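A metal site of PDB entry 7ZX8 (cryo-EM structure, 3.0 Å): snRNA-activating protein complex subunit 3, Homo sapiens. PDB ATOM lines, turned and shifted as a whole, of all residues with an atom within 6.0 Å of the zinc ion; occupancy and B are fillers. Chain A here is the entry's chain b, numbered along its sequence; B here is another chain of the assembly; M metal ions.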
ATOM      1  N   CYS A 354      -3.338 -22.946   3.061  1.00  0.00           N
ATOM      2  CA  CYS A 354      -4.581 -23.590   2.657  1.00  0.00           C
ATOM      3  C   CYS A 354      -5.602 -23.486   3.774  1.00  0.00           C
ATOM      4  O   CYS A 354      -5.272 -23.363   4.955  1.00  0.00           O
ATOM      5  CB  CYS A 354      -4.333 -25.058   2.314  1.00  0.00           C
ATOM      6  SG  CYS A 354      -5.803 -26.078   2.193  1.00  0.00           S
ATOM      7  N   PHE A 355      -6.887 -23.530   3.398  1.00  0.00           N
ATOM      8  CA  PHE A 355      -7.947 -23.368   4.373  1.00  0.00           C
ATOM      9  C   PHE A 355      -8.491 -24.686   4.884  1.00  0.00           C
ATOM     10  O   PHE A 355      -9.035 -24.735   5.980  1.00  0.00           O
ATOM     11  CB  PHE A 355      -9.071 -22.515   3.805  1.00  0.00           C
ATOM     12  CG  PHE A 355      -8.873 -21.056   4.029  1.00  0.00           C
ATOM     13  CD1 PHE A 355      -7.602 -20.546   4.239  1.00  0.00           C
ATOM     14  CD2 PHE A 355      -9.952 -20.195   4.034  1.00  0.00           C
ATOM     15  CE1 PHE A 355      -7.414 -19.201   4.441  1.00  0.00           C
ATOM     16  CE2 PHE A 355      -9.767 -18.846   4.246  1.00  0.00           C
ATOM     17  CZ  PHE A 355      -8.495 -18.352   4.452  1.00  0.00           C
ATOM     18  N   VAL A 356      -8.365 -25.753   4.104  1.00  0.00           N
ATOM     19  CA  VAL A 356      -8.758 -27.083   4.547  1.00  0.00           C
ATOM     20  C   VAL A 356      -7.697 -27.677   5.460  1.00  0.00           C
ATOM     21  O   VAL A 356      -7.973 -27.952   6.633  1.00  0.00           O
ATOM     22  CB  VAL A 356      -9.020 -28.009   3.342  1.00  0.00           C
ATOM     23  CG1 VAL A 356      -9.728 -29.256   3.812  1.00  0.00           C
ATOM     24  CG2 VAL A 356      -9.824 -27.290   2.302  1.00  0.00           C
ATOM     25  N   CYS A 357      -6.494 -27.873   4.950  1.00  0.00           N
ATOM     26  CA  CYS A 357      -5.349 -28.257   5.765  1.00  0.00           C
ATOM     27  C   CYS A 357      -4.500 -27.019   5.978  1.00  0.00           C
ATOM     28  O   CYS A 357      -4.542 -26.084   5.172  1.00  0.00           O
ATOM     29  CB  CYS A 357      -4.533 -29.354   5.086  1.00  0.00           C
ATOM     30  SG  CYS A 357      -3.996 -28.891   3.438  1.00  0.00           S
ATOM     31  N   LYS A 358      -3.740 -27.010   7.060  1.00  0.00           N
ATOM     32  CA  LYS A 358      -2.878 -25.878   7.381  1.00  0.00           C
ATOM     33  C   LYS A 358      -1.407 -26.214   7.209  1.00  0.00           C
ATOM     34  O   LYS A 358      -0.537 -25.555   7.777  1.00  0.00           O
ATOM     35  CB  LYS A 358      -3.147 -25.387   8.791  1.00  0.00           C
ATOM     36  CG  LYS A 358      -4.588 -25.021   9.052  1.00  0.00           C
ATOM     37  CD  LYS A 358      -5.098 -24.126   7.954  1.00  0.00           C
ATOM     38  CE  LYS A 358      -6.273 -23.291   8.442  1.00  0.00           C
ATOM     39  NZ  LYS A 358      -5.844 -22.336   9.496  1.00  0.00           N
ATOM     40  N   TYR A 360       0.239 -26.456   4.156  1.00  0.00           N
ATOM     41  CA  TYR A 360       0.786 -26.025   2.881  1.00  0.00           C
ATOM     42  C   TYR A 360       0.267 -24.642   2.561  1.00  0.00           C
ATOM     43  O   TYR A 360      -0.623 -24.112   3.247  1.00  0.00           O
ATOM     44  CB  TYR A 360       0.449 -27.014   1.759  1.00  0.00           C
ATOM     45  CG  TYR A 360       0.852 -28.430   2.065  1.00  0.00           C
ATOM     46  CD1 TYR A 360       2.105 -28.901   1.695  1.00  0.00           C
ATOM     47  CD2 TYR A 360       0.001 -29.296   2.730  1.00  0.00           C
ATOM     48  CE1 TYR A 360       2.480 -30.191   1.981  1.00  0.00           C
ATOM     49  CE2 TYR A 360       0.381 -30.575   3.025  1.00  0.00           C
ATOM     50  CZ  TYR A 360       1.614 -31.022   2.648  1.00  0.00           C
ATOM     51  OH  TYR A 360       1.997 -32.305   2.935  1.00  0.00           O
ATOM     52  N   PHE A 379      -6.936 -22.543  -1.181  1.00  0.00           N
ATOM     53  CA  PHE A 379      -6.698 -23.970  -1.110  1.00  0.00           C
ATOM     54  C   PHE A 379      -5.297 -24.279  -1.593  1.00  0.00           C
ATOM     55  O   PHE A 379      -4.862 -23.753  -2.628  1.00  0.00           O
ATOM     56  CB  PHE A 379      -7.698 -24.748  -1.956  1.00  0.00           C
ATOM     57  CG  PHE A 379      -9.117 -24.576  -1.534  1.00  0.00           C
ATOM     58  CD1 PHE A 379      -9.723 -25.513  -0.719  1.00  0.00           C
ATOM     59  CD2 PHE A 379      -9.854 -23.496  -1.955  1.00  0.00           C
ATOM     60  CE1 PHE A 379     -11.025 -25.374  -0.333  1.00  0.00           C
ATOM     61  CE2 PHE A 379     -11.162 -23.350  -1.574  1.00  0.00           C
ATOM     62  CZ  PHE A 379     -11.747 -24.282  -0.754  1.00  0.00           C
ATOM     63  N   CYS A 380      -4.589 -25.125  -0.861  1.00  0.00           N
ATOM     64  CA  CYS A 380      -3.398 -25.746  -1.405  1.00  0.00           C
ATOM     65  C   CYS A 380      -3.773 -26.629  -2.586  1.00  0.00           C
ATOM     66  O   CYS A 380      -4.937 -27.001  -2.752  1.00  0.00           O
ATOM     67  CB  CYS A 380      -2.693 -26.580  -0.347  1.00  0.00           C
ATOM     68  SG  CYS A 380      -3.661 -27.981   0.194  1.00  0.00           S
ATOM     69  N   ASP A 381      -2.784 -26.968  -3.392  1.00  0.00           N
ATOM     70  CA  ASP A 381      -3.077 -27.715  -4.606  1.00  0.00           C
ATOM     71  C   ASP A 381      -3.645 -29.088  -4.285  1.00  0.00           C
ATOM     72  O   ASP A 381      -4.556 -29.578  -4.965  1.00  0.00           O
ATOM     73  CB  ASP A 381      -1.818 -27.832  -5.463  1.00  0.00           C
ATOM     74  CG  ASP A 381      -2.133 -28.123  -6.910  1.00  0.00           C
ATOM     75  OD1 ASP A 381      -2.604 -27.200  -7.606  1.00  0.00           O
ATOM     76  OD2 ASP A 381      -1.925 -29.263  -7.353  1.00  0.00           O
ATOM     77  N   VAL A 382      -3.138 -29.715  -3.226  1.00  0.00           N
ATOM     78  CA  VAL A 382      -3.588 -31.057  -2.855  1.00  0.00           C
ATOM     79  C   VAL A 382      -5.096 -31.082  -2.662  1.00  0.00           C
ATOM     80  O   VAL A 382      -5.821 -31.780  -3.370  1.00  0.00           O
ATOM     81  CB  VAL A 382      -2.856 -31.542  -1.599  1.00  0.00           C
ATOM     82  CG1 VAL A 382      -3.482 -32.824  -1.086  1.00  0.00           C
ATOM     83  CG2 VAL A 382      -1.382 -31.744  -1.898  1.00  0.00           C
ATOM     84  N   CYS A 383      -5.586 -30.307  -1.695  1.00  0.00           N
ATOM     85  CA  CYS A 383      -7.011 -30.366  -1.377  1.00  0.00           C
ATOM     86  C   CYS A 383      -7.856 -29.708  -2.451  1.00  0.00           C
ATOM     87  O   CYS A 383      -8.975 -30.154  -2.729  1.00  0.00           O
ATOM     88  CB  CYS A 383      -7.267 -29.735  -0.014  1.00  0.00           C
ATOM     89  SG  CYS A 383      -6.103 -30.286   1.247  1.00  0.00           S
ATOM     90  N   PHE A 384      -7.341 -28.641  -3.068  1.00  0.00           N
ATOM     91  CA  PHE A 384      -8.045 -28.061  -4.208  1.00  0.00           C
ATOM     92  C   PHE A 384      -8.356 -29.111  -5.259  1.00  0.00           C
ATOM     93  O   PHE A 384      -9.417 -29.088  -5.885  1.00  0.00           O
ATOM     94  CB  PHE A 384      -7.221 -26.941  -4.822  1.00  0.00           C
ATOM     95  CG  PHE A 384      -7.778 -26.434  -6.108  1.00  0.00           C
ATOM     96  CD1 PHE A 384      -8.884 -25.619  -6.115  1.00  0.00           C
ATOM     97  CD2 PHE A 384      -7.201 -26.789  -7.301  1.00  0.00           C
ATOM     98  CE1 PHE A 384      -9.405 -25.151  -7.291  1.00  0.00           C
ATOM     99  CE2 PHE A 384      -7.712 -26.318  -8.486  1.00  0.00           C
ATOM    100  CZ  PHE A 384      -8.820 -25.499  -8.484  1.00  0.00           C
ATOM    101  N   GLN B 338      -8.086 -34.663   6.504  1.00  0.00           N
ATOM    102  CA  GLN B 338      -6.713 -34.175   6.381  1.00  0.00           C
ATOM    103  C   GLN B 338      -6.028 -34.099   7.740  1.00  0.00           C
ATOM    104  O   GLN B 338      -4.897 -34.565   7.887  1.00  0.00           O
ATOM    105  CB  GLN B 338      -6.713 -32.801   5.715  1.00  0.00           C
ATOM    106  CG  GLN B 338      -7.279 -32.802   4.319  1.00  0.00           C
ATOM    107  CD  GLN B 338      -6.382 -33.490   3.326  1.00  0.00           C
ATOM    108  OE1 GLN B 338      -6.502 -34.698   3.109  1.00  0.00           O
ATOM    109  NE2 GLN B 338      -5.494 -32.731   2.699  1.00  0.00           N
HETATM  110 ZN    ZN M   1      -5.225 -28.201   1.600  1.00  0.00          ZN
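The side-chain sulfur (SG) of Cys 354 lies close to the backbone NH (N) of Val 356 (3.2 Å).
SG of Cys 383 lies close to NE2 of Gln 338 of chain B (2.9 Å).
The backbone NH of Cys 354 sits at hydrogen-bond distance from the backbone carbonyl oxygen of Tyr 360 (3.0 Å).
Four residues have an atom within 4 Å of the zinc ion: Cys 354, Cys 357, Cys 380 and Cys 383.
The nearest printed residue that does not touch the zinc ion is Val 356 (4.2 Å).
The zinc ion is bound by SG of Cys 380, SG of Cys 354, SG of Cys 383 and SG of Cys 357.
The zinc ion has four donor atoms within binding distance.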
